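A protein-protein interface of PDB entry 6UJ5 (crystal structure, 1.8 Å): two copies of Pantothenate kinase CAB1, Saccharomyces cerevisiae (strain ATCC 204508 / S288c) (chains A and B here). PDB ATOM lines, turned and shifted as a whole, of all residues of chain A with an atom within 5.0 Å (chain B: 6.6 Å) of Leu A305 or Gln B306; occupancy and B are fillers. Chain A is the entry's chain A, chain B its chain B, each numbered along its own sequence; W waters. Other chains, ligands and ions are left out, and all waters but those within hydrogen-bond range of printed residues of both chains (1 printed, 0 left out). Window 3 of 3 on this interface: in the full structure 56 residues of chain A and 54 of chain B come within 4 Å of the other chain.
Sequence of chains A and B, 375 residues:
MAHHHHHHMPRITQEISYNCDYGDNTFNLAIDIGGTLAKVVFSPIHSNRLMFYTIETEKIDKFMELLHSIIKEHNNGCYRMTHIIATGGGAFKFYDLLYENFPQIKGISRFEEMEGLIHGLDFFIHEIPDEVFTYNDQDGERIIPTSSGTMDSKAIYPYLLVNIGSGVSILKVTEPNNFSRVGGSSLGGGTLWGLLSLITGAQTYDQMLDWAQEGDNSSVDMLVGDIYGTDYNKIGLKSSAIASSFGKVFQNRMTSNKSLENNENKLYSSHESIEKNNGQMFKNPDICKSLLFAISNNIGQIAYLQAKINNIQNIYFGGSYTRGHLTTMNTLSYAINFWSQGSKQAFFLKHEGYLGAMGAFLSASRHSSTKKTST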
ATOM      1  N   GLY A 300     -23.934   5.700  -8.526  1.00  0.00           N
ATOM      2  CA  GLY A 300     -25.234   6.339  -8.698  1.00  0.00           C
ATOM      3  C   GLY A 300     -25.623   6.518 -10.152  1.00  0.00           C
ATOM      4  O   GLY A 300     -26.788   6.329 -10.523  1.00  0.00           O
ATOM      5  N   GLN A 301     -24.666   6.903 -11.000  1.00  0.00           N
ATOM      6  CA  GLN A 301     -24.968   7.014 -12.427  1.00  0.00           C
ATOM      7  C   GLN A 301     -25.326   5.661 -13.033  1.00  0.00           C
ATOM      8  O   GLN A 301     -26.321   5.539 -13.755  1.00  0.00           O
ATOM      9  CB  GLN A 301     -23.790   7.613 -13.189  1.00  0.00           C
ATOM     10  CG  GLN A 301     -24.118   7.802 -14.674  1.00  0.00           C
ATOM     11  CD  GLN A 301     -23.041   8.545 -15.429  1.00  0.00           C
ATOM     12  OE1 GLN A 301     -21.905   8.635 -14.974  1.00  0.00           O
ATOM     13  NE2 GLN A 301     -23.398   9.096 -16.585  1.00  0.00           N
ATOM     14  N   ILE A 302     -24.507   4.632 -12.784  1.00  0.00           N
ATOM     15  CA  ILE A 302     -24.822   3.331 -13.360  1.00  0.00           C
ATOM     16  C   ILE A 302     -26.166   2.831 -12.840  1.00  0.00           C
ATOM     17  O   ILE A 302     -26.970   2.284 -13.610  1.00  0.00           O
ATOM     18  CB  ILE A 302     -23.679   2.335 -13.099  1.00  0.00           C
ATOM     19  CG1 ILE A 302     -22.496   2.695 -14.002  1.00  0.00           C
ATOM     20  CG2 ILE A 302     -24.113   0.890 -13.379  1.00  0.00           C
ATOM     21  CD1 ILE A 302     -21.236   1.938 -13.654  1.00  0.00           C
ATOM     22  N   ALA A 303     -26.446   3.048 -11.557  1.00  0.00           N
ATOM     23  CA  ALA A 303     -27.741   2.666 -10.996  1.00  0.00           C
ATOM     24  C   ALA A 303     -28.869   3.419 -11.676  1.00  0.00           C
ATOM     25  O   ALA A 303     -29.918   2.836 -11.995  1.00  0.00           O
ATOM     26  CB  ALA A 303     -27.761   2.937  -9.492  1.00  0.00           C
ATOM     27  N   TYR A 304     -28.672   4.717 -11.906  1.00  0.00           N
ATOM     28  CA  TYR A 304     -29.688   5.497 -12.598  1.00  0.00           C
ATOM     29  C   TYR A 304     -29.930   4.956 -13.998  1.00  0.00           C
ATOM     30  O   TYR A 304     -31.078   4.796 -14.429  1.00  0.00           O
ATOM     31  CB  TYR A 304     -29.268   6.962 -12.670  1.00  0.00           C
ATOM     32  CG  TYR A 304     -30.060   7.690 -13.711  1.00  0.00           C
ATOM     33  CD1 TYR A 304     -31.379   8.062 -13.462  1.00  0.00           C
ATOM     34  CD2 TYR A 304     -29.516   7.978 -14.958  1.00  0.00           C
ATOM     35  CE1 TYR A 304     -32.119   8.703 -14.406  1.00  0.00           C
ATOM     36  CE2 TYR A 304     -30.274   8.634 -15.923  1.00  0.00           C
ATOM     37  CZ  TYR A 304     -31.562   8.988 -15.635  1.00  0.00           C
ATOM     38  OH  TYR A 304     -32.308   9.634 -16.588  1.00  0.00           O
ATOM     39  N   LEU A 305     -28.856   4.708 -14.740  1.00  0.00           N
ATOM     40  CA  LEU A 305     -29.013   4.266 -16.120  1.00  0.00           C
ATOM     41  C   LEU A 305     -29.702   2.903 -16.188  1.00  0.00           C
ATOM     42  O   LEU A 305     -30.564   2.678 -17.048  1.00  0.00           O
ATOM     43  CB  LEU A 305     -27.655   4.235 -16.815  1.00  0.00           C
ATOM     44  CG  LEU A 305     -26.995   5.614 -17.002  1.00  0.00           C
ATOM     45  CD1 LEU A 305     -25.550   5.415 -17.421  1.00  0.00           C
ATOM     46  CD2 LEU A 305     -27.741   6.459 -18.026  1.00  0.00           C
ATOM     47  N   GLN A 306     -29.374   1.997 -15.261  1.00  0.00           N
ATOM     48  CA  GLN A 306     -30.075   0.716 -15.234  1.00  0.00           C
ATOM     49  C   GLN A 306     -31.545   0.895 -14.865  1.00  0.00           C
ATOM     50  O   GLN A 306     -32.412   0.207 -15.413  1.00  0.00           O
ATOM     51  CB  GLN A 306     -29.398  -0.254 -14.263  1.00  0.00           C
ATOM     52  CG  GLN A 306     -27.990  -0.728 -14.684  1.00  0.00           C
ATOM     53  CD  GLN A 306     -28.018  -1.769 -15.799  1.00  0.00           C
ATOM     54  OE1 GLN A 306     -29.009  -1.897 -16.512  1.00  0.00           O
ATOM     55  NE2 GLN A 306     -26.938  -2.533 -15.935  1.00  0.00           N
ATOM     56  N   ALA A 307     -31.848   1.794 -13.929  1.00  0.00           N
ATOM     57  CA  ALA A 307     -33.253   2.037 -13.598  1.00  0.00           C
ATOM     58  C   ALA A 307     -33.990   2.654 -14.774  1.00  0.00           C
ATOM     59  O   ALA A 307     -35.178   2.373 -15.003  1.00  0.00           O
ATOM     60  CB  ALA A 307     -33.359   2.933 -12.367  1.00  0.00           C
ATOM     61  N   LYS A 308     -33.294   3.480 -15.551  1.00  0.00           N
ATOM     62  CA  LYS A 308     -33.897   4.090 -16.732  1.00  0.00           C
ATOM     63  C   LYS A 308     -34.214   3.036 -17.792  1.00  0.00           C
ATOM     64  O   LYS A 308     -35.332   2.987 -18.332  1.00  0.00           O
ATOM     65  CB  LYS A 308     -32.942   5.165 -17.284  1.00  0.00           C
ATOM     66  CG  LYS A 308     -33.600   6.160 -18.220  1.00  0.00           C
ATOM     67  CD  LYS A 308     -34.513   7.118 -17.453  1.00  0.00           C
ATOM     68  CE  LYS A 308     -35.394   7.945 -18.387  1.00  0.00           C
ATOM     69  NZ  LYS A 308     -34.589   8.740 -19.352  1.00  0.00           N
ATOM     70  N   ILE A 309     -33.248   2.158 -18.072  1.00  0.00           N
ATOM     71  CA  ILE A 309     -33.440   1.065 -19.027  1.00  0.00           C
ATOM     72  C   ILE A 309     -34.606   0.170 -18.614  1.00  0.00           C
ATOM     73  O   ILE A 309     -35.380  -0.304 -19.459  1.00  0.00           O
ATOM     74  CB  ILE A 309     -32.139   0.254 -19.156  1.00  0.00           C
ATOM     75  CG1 ILE A 309     -31.076   1.071 -19.888  1.00  0.00           C
ATOM     76  CG2 ILE A 309     -32.382  -1.055 -19.895  1.00  0.00           C
ATOM     77  CD1 ILE A 309     -29.689   0.458 -19.804  1.00  0.00           C
ATOM     78  N   LEU B 160     -22.996   7.194 -31.383  1.00  0.00           N
ATOM     79  CA  LEU B 160     -22.605   7.838 -30.152  1.00  0.00           C
ATOM     80  C   LEU B 160     -21.140   8.191 -30.295  1.00  0.00           C
ATOM     81  O   LEU B 160     -20.360   7.393 -30.824  1.00  0.00           O
ATOM     82  CB  LEU B 160     -22.795   6.873 -28.965  1.00  0.00           C
ATOM     83  CG  LEU B 160     -23.146   7.296 -27.552  1.00  0.00           C
ATOM     84  CD1 LEU B 160     -24.531   7.910 -27.524  1.00  0.00           C
ATOM     85  CD2 LEU B 160     -23.065   6.081 -26.622  1.00  0.00           C
ATOM     86  N   ILE B 170     -20.211  12.458 -23.777  1.00  0.00           N
ATOM     87  CA  ILE B 170     -20.919  11.510 -24.634  1.00  0.00           C
ATOM     88  C   ILE B 170     -21.961  12.291 -25.413  1.00  0.00           C
ATOM     89  O   ILE B 170     -22.793  12.983 -24.816  1.00  0.00           O
ATOM     90  CB  ILE B 170     -21.572  10.365 -23.845  1.00  0.00           C
ATOM     91  CG1 ILE B 170     -20.512   9.653 -23.000  1.00  0.00           C
ATOM     92  CG2 ILE B 170     -22.218   9.370 -24.800  1.00  0.00           C
ATOM     93  CD1 ILE B 170     -21.073   8.469 -22.216  1.00  0.00           C
ATOM     94  N   VAL B 182     -25.530  13.640 -23.914  1.00  0.00           N
ATOM     95  CA  VAL B 182     -26.143  12.820 -22.869  1.00  0.00           C
ATOM     96  C   VAL B 182     -25.164  12.712 -21.701  1.00  0.00           C
ATOM     97  O   VAL B 182     -24.037  13.213 -21.772  1.00  0.00           O
ATOM     98  CB  VAL B 182     -26.576  11.427 -23.383  1.00  0.00           C
ATOM     99  CG1 VAL B 182     -27.625  11.553 -24.483  1.00  0.00           C
ATOM    100  CG2 VAL B 182     -25.396  10.604 -23.871  1.00  0.00           C
ATOM    101  N   GLY B 183     -25.593  12.080 -20.614  1.00  0.00           N
ATOM    102  CA  GLY B 183     -24.756  11.982 -19.435  1.00  0.00           C
ATOM    103  C   GLY B 183     -23.396  11.354 -19.668  1.00  0.00           C
ATOM    104  O   GLY B 183     -23.291  10.235 -20.178  1.00  0.00           O
ATOM    105  N   GLY B 184     -22.346  12.068 -19.287  1.00  0.00           N
ATOM    106  CA  GLY B 184     -20.984  11.582 -19.369  1.00  0.00           C
ATOM    107  C   GLY B 184     -20.476  11.091 -18.027  1.00  0.00           C
ATOM    108  O   GLY B 184     -21.238  10.594 -17.194  1.00  0.00           O
ATOM    109  N   GLN B 301     -18.755   0.471 -20.210  1.00  0.00           N
ATOM    110  CA  GLN B 301     -20.080   0.153 -19.685  1.00  0.00           C
ATOM    111  C   GLN B 301     -21.026   1.346 -19.782  1.00  0.00           C
ATOM    112  O   GLN B 301     -22.188   1.185 -20.170  1.00  0.00           O
ATOM    113  CB  GLN B 301     -19.991  -0.325 -18.231  1.00  0.00           C
ATOM    114  CG  GLN B 301     -21.385  -0.627 -17.653  1.00  0.00           C
ATOM    115  CD  GLN B 301     -21.348  -1.286 -16.293  1.00  0.00           C
ATOM    116  OE1 GLN B 301     -20.375  -1.163 -15.555  1.00  0.00           O
ATOM    117  NE2 GLN B 301     -22.409  -2.001 -15.960  1.00  0.00           N
ATOM    118  N   ILE B 302     -20.567   2.543 -19.412  1.00  0.00           N
ATOM    119  CA  ILE B 302     -21.437   3.712 -19.491  1.00  0.00           C
ATOM    120  C   ILE B 302     -21.805   4.011 -20.938  1.00  0.00           C
ATOM    121  O   ILE B 302     -22.952   4.369 -21.235  1.00  0.00           O
ATOM    122  CB  ILE B 302     -20.780   4.921 -18.803  1.00  0.00           C
ATOM    123  CG1 ILE B 302     -20.705   4.639 -17.297  1.00  0.00           C
ATOM    124  CG2 ILE B 302     -21.590   6.190 -19.064  1.00  0.00           C
ATOM    125  CD1 ILE B 302     -20.026   5.688 -16.488  1.00  0.00           C
ATOM    126  N   ALA B 303     -20.848   3.851 -21.856  1.00  0.00           N
ATOM    127  CA  ALA B 303     -21.129   3.986 -23.287  1.00  0.00           C
ATOM    128  C   ALA B 303     -22.178   2.985 -23.733  1.00  0.00           C
ATOM    129  O   ALA B 303     -23.127   3.336 -24.450  1.00  0.00           O
ATOM    130  CB  ALA B 303     -19.843   3.789 -24.099  1.00  0.00           C
ATOM    131  N   TYR B 304     -22.026   1.726 -23.307  1.00  0.00           N
ATOM    132  CA  TYR B 304     -23.002   0.701 -23.637  1.00  0.00           C
ATOM    133  C   TYR B 304     -24.385   1.079 -23.129  1.00  0.00           C
ATOM    134  O   TYR B 304     -25.385   0.928 -23.844  1.00  0.00           O
ATOM    135  CB  TYR B 304     -22.589  -0.649 -23.048  1.00  0.00           C
ATOM    136  CG  TYR B 304     -23.769  -1.563 -23.047  1.00  0.00           C
ATOM    137  CD1 TYR B 304     -24.198  -2.136 -24.232  1.00  0.00           C
ATOM    138  CD2 TYR B 304     -24.496  -1.810 -21.884  1.00  0.00           C
ATOM    139  CE1 TYR B 304     -25.307  -2.956 -24.263  1.00  0.00           C
ATOM    140  CE2 TYR B 304     -25.611  -2.650 -21.915  1.00  0.00           C
ATOM    141  CZ  TYR B 304     -26.002  -3.204 -23.108  1.00  0.00           C
ATOM    142  OH  TYR B 304     -27.108  -4.028 -23.162  1.00  0.00           O
ATOM    143  N   LEU B 305     -24.463   1.543 -21.877  1.00  0.00           N
ATOM    144  CA  LEU B 305     -25.764   1.845 -21.288  1.00  0.00           C
ATOM    145  C   LEU B 305     -26.415   3.026 -21.990  1.00  0.00           C
ATOM    146  O   LEU B 305     -27.627   3.018 -22.237  1.00  0.00           O
ATOM    147  CB  LEU B 305     -25.626   2.119 -19.788  1.00  0.00           C
ATOM    148  CG  LEU B 305     -25.216   0.903 -18.938  1.00  0.00           C
ATOM    149  CD1 LEU B 305     -24.799   1.346 -17.525  1.00  0.00           C
ATOM    150  CD2 LEU B 305     -26.354  -0.089 -18.842  1.00  0.00           C
ATOM    151  N   GLN B 306     -25.627   4.040 -22.345  1.00  0.00           N
ATOM    152  CA  GLN B 306     -26.220   5.150 -23.082  1.00  0.00           C
ATOM    153  C   GLN B 306     -26.675   4.706 -24.470  1.00  0.00           C
ATOM    154  O   GLN B 306     -27.700   5.174 -24.978  1.00  0.00           O
ATOM    155  CB  GLN B 306     -25.234   6.309 -23.161  1.00  0.00           C
ATOM    156  CG  GLN B 306     -24.939   6.953 -21.800  1.00  0.00           C
ATOM    157  CD  GLN B 306     -26.083   7.804 -21.274  1.00  0.00           C
ATOM    158  OE1 GLN B 306     -27.251   7.552 -21.575  1.00  0.00           O
ATOM    159  NE2 GLN B 306     -25.751   8.803 -20.464  1.00  0.00           N
ATOM    160  N   ALA B 307     -25.916   3.813 -25.101  1.00  0.00           N
ATOM    161  CA  ALA B 307     -26.298   3.332 -26.425  1.00  0.00           C
ATOM    162  C   ALA B 307     -27.536   2.452 -26.349  1.00  0.00           C
ATOM    163  O   ALA B 307     -28.392   2.483 -27.247  1.00  0.00           O
ATOM    164  CB  ALA B 307     -25.128   2.582 -27.057  1.00  0.00           C
ATOM    165  N   LYS B 308     -27.655   1.674 -25.274  1.00  0.00           N
ATOM    166  CA  LYS B 308     -28.853   0.868 -25.059  1.00  0.00           C
ATOM    167  C   LYS B 308     -30.078   1.757 -24.927  1.00  0.00           C
ATOM    168  O   LYS B 308     -31.120   1.513 -25.553  1.00  0.00           O
ATOM    169  CB  LYS B 308     -28.667   0.019 -23.799  1.00  0.00           C
ATOM    170  CG  LYS B 308     -29.848  -0.868 -23.446  1.00  0.00           C
ATOM    171  CD  LYS B 308     -29.930  -2.052 -24.391  1.00  0.00           C
ATOM    172  CE  LYS B 308     -30.983  -3.050 -23.924  1.00  0.00           C
ATOM    173  NZ  LYS B 308     -31.024  -4.282 -24.769  1.00  0.00           N
ATOM    174  N   ILE B 309     -29.968   2.788 -24.090  1.00  0.00           N
ATOM    175  CA  ILE B 309     -31.081   3.700 -23.835  1.00  0.00           C
ATOM    176  C   ILE B 309     -31.522   4.370 -25.120  1.00  0.00           C
ATOM    177  O   ILE B 309     -32.723   4.576 -25.354  1.00  0.00           O
ATOM    178  CB  ILE B 309     -30.665   4.733 -22.769  1.00  0.00           C
ATOM    179  CG1 ILE B 309     -30.612   4.068 -21.392  1.00  0.00           C
ATOM    180  CG2 ILE B 309     -31.596   5.947 -22.761  1.00  0.00           C
ATOM    181  CD1 ILE B 309     -30.018   4.964 -20.315  1.00  0.00           C
ATOM    182  N   ASN B 310     -30.572   4.688 -25.986  1.00  0.00           N
ATOM    183  CA  ASN B 310     -30.846   5.454 -27.193  1.00  0.00           C
ATOM    184  C   ASN B 310     -30.924   4.587 -28.452  1.00  0.00           C
ATOM    185  O   ASN B 310     -30.940   5.129 -29.566  1.00  0.00           O
ATOM    186  CB  ASN B 310     -29.793   6.551 -27.335  1.00  0.00           C
ATOM    187  CG  ASN B 310     -29.937   7.623 -26.261  1.00  0.00           C
ATOM    188  OD1 ASN B 310     -30.882   8.404 -26.290  1.00  0.00           O
ATOM    189  ND2 ASN B 310     -29.008   7.658 -25.308  1.00  0.00           N
ATOM    190  N   ASN B 311     -31.011   3.262 -28.292  1.00  0.00           N
ATOM    191  CA  ASN B 311     -31.067   2.297 -29.398  1.00  0.00           C
ATOM    192  C   ASN B 311     -30.053   2.623 -30.496  1.00  0.00           C
ATOM    193  O   ASN B 311     -30.391   2.835 -31.661  1.00  0.00           O
ATOM    194  CB  ASN B 311     -32.479   2.207 -29.987  1.00  0.00           C
ATOM    195  CG  ASN B 311     -32.656   0.976 -30.855  1.00  0.00           C
ATOM    196  OD1 ASN B 311     -32.048  -0.065 -30.598  1.00  0.00           O
ATOM    197  ND2 ASN B 311     -33.476   1.089 -31.897  1.00  0.00           N
ATOM    198  N   ILE B 312     -28.790   2.682 -30.094  1.00  0.00           N
ATOM    199  CA  ILE B 312     -27.676   3.000 -30.979  1.00  0.00           C
ATOM    200  C   ILE B 312     -26.730   1.809 -30.987  1.00  0.00           C
ATOM    201  O   ILE B 312     -26.439   1.240 -29.928  1.00  0.00           O
ATOM    202  CB  ILE B 312     -26.946   4.270 -30.503  1.00  0.00           C
ATOM    203  CG1 ILE B 312     -27.810   5.509 -30.765  1.00  0.00           C
ATOM    204  CG2 ILE B 312     -25.565   4.398 -31.160  1.00  0.00           C
ATOM    205  CD1 ILE B 312     -27.232   6.772 -30.147  1.00  0.00           C
ATOM    206  N   LYS B 344     -23.624  -4.302 -30.514  1.00  0.00           N
ATOM    207  CA  LYS B 344     -23.038  -2.978 -30.627  1.00  0.00           C
ATOM    208  C   LYS B 344     -21.545  -3.112 -30.885  1.00  0.00           C
ATOM    209  O   LYS B 344     -20.935  -4.142 -30.581  1.00  0.00           O
ATOM    210  CB  LYS B 344     -23.296  -2.143 -29.367  1.00  0.00           C
ATOM    211  CG  LYS B 344     -24.784  -2.057 -28.992  1.00  0.00           C
ATOM    212  CD  LYS B 344     -25.056  -0.993 -27.916  1.00  0.00           C
ATOM    213  CE  LYS B 344     -26.492  -1.118 -27.379  1.00  0.00           C
ATOM    214  NZ  LYS B 344     -27.559  -0.917 -28.430  1.00  0.00           N
HETATM  215  O   HOH W   1     -21.187  11.156 -14.065  1.00  0.00           O
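The side-chain amide nitrogen (NE2) of Gln A301 sits at hydrogen-bond distance from the backbone carbonyl oxygen (O) of Gly B184 (2.7 Å).
The backbone carbonyl oxygen (O) of Gly B183 lies within hydrogen-bond range of the side-chain amide nitrogen (NE2) of Gln B306 (2.9 Å). ND2 of Asn B310 lies within hydrogen-bond range of O of Gln B306, 2.8 Å away.
Gly B183 touches Gln A301 (O to NE2, 3.8 Å). Ile B302 touches Gln A301 (CD1 to OE1, 3.8 Å). Ile A302 touches Gln B301. Leu A305 touches Gln B306 (CD2 to OE1, 3.7 Å). Leu A305 touches Ile B309. Leu B305 touches Gln A306 (CD2 to NE2, 3.8 Å). Ile A309 touches Leu B305 (CD1 to CD2, 3.5 Å). CD1 of Ile A309 touches CG of Lys B308 (3.9 Å). Ile B309 touches Ile A309.
Gln B306 touches one residue of chain A. Of the printed residues of chain A, Gly B184 touches Gln A301. Of the printed residues of chain B, Gln A301 touches Gly B183 (3.8 Å), Gly B184 (2.7 Å) and Ile B302 (3.8 Å). Printed residues of chain A within 4 Å of Gln B301: Ile A302 (3.7 Å). Ala A307 touches none of the printed residues of chain B. The nearest residue of chain B that does not touch Leu A305 is Leu B305 (4.1 Å). The nearest printed residue of chain A that does not touch Ile B302 is Ile A302 (4.2 Å).
Of the 18 printed residues of chain B, 8 touch a printed residue of chain A. Printed residues of chain B that touch a printed residue of chain A: Gly B183, Gly B184, Gln B301, Ile B302, Leu B305, Gln B306, Lys B308 and Ile B309. Hydrophobic or aromatic side chains of chain B within 4 Å of the printed part of chain A: Ile B302, Leu B305 and Ile B309. Along chain B the printed residues that touch a printed residue of chain A span positions 183 to 309. Among the printed residues, 10 pairs touch across the chains. Among the printed residues, no Asp or Glu carboxylate lies within 4 Å of a Lys or Arg side-chain nitrogen of the other chain.
Leu A305 touches Gln B306, and with the chains exchanged Gln A306 touches Leu B305. Leu A305 touches Ile B309, and with the chains exchanged Ile A309 touches Leu B305. Ile A309 touches Lys B308, but with the chains exchanged Lys A308 does not touch Ile B309 (4.2 Å). Ile A309 touches its own counterpart, Ile B309. Positions printed for both chains: 301, 302, 303, 304, 305, 306, 307, 308 and 309. Of the 10 pairs that touch across the chains among the printed residues, 7 have their exchanged pair printed and touching as well.
Water W1 bridges OE1 of Gln A301 and O of Gly B184.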
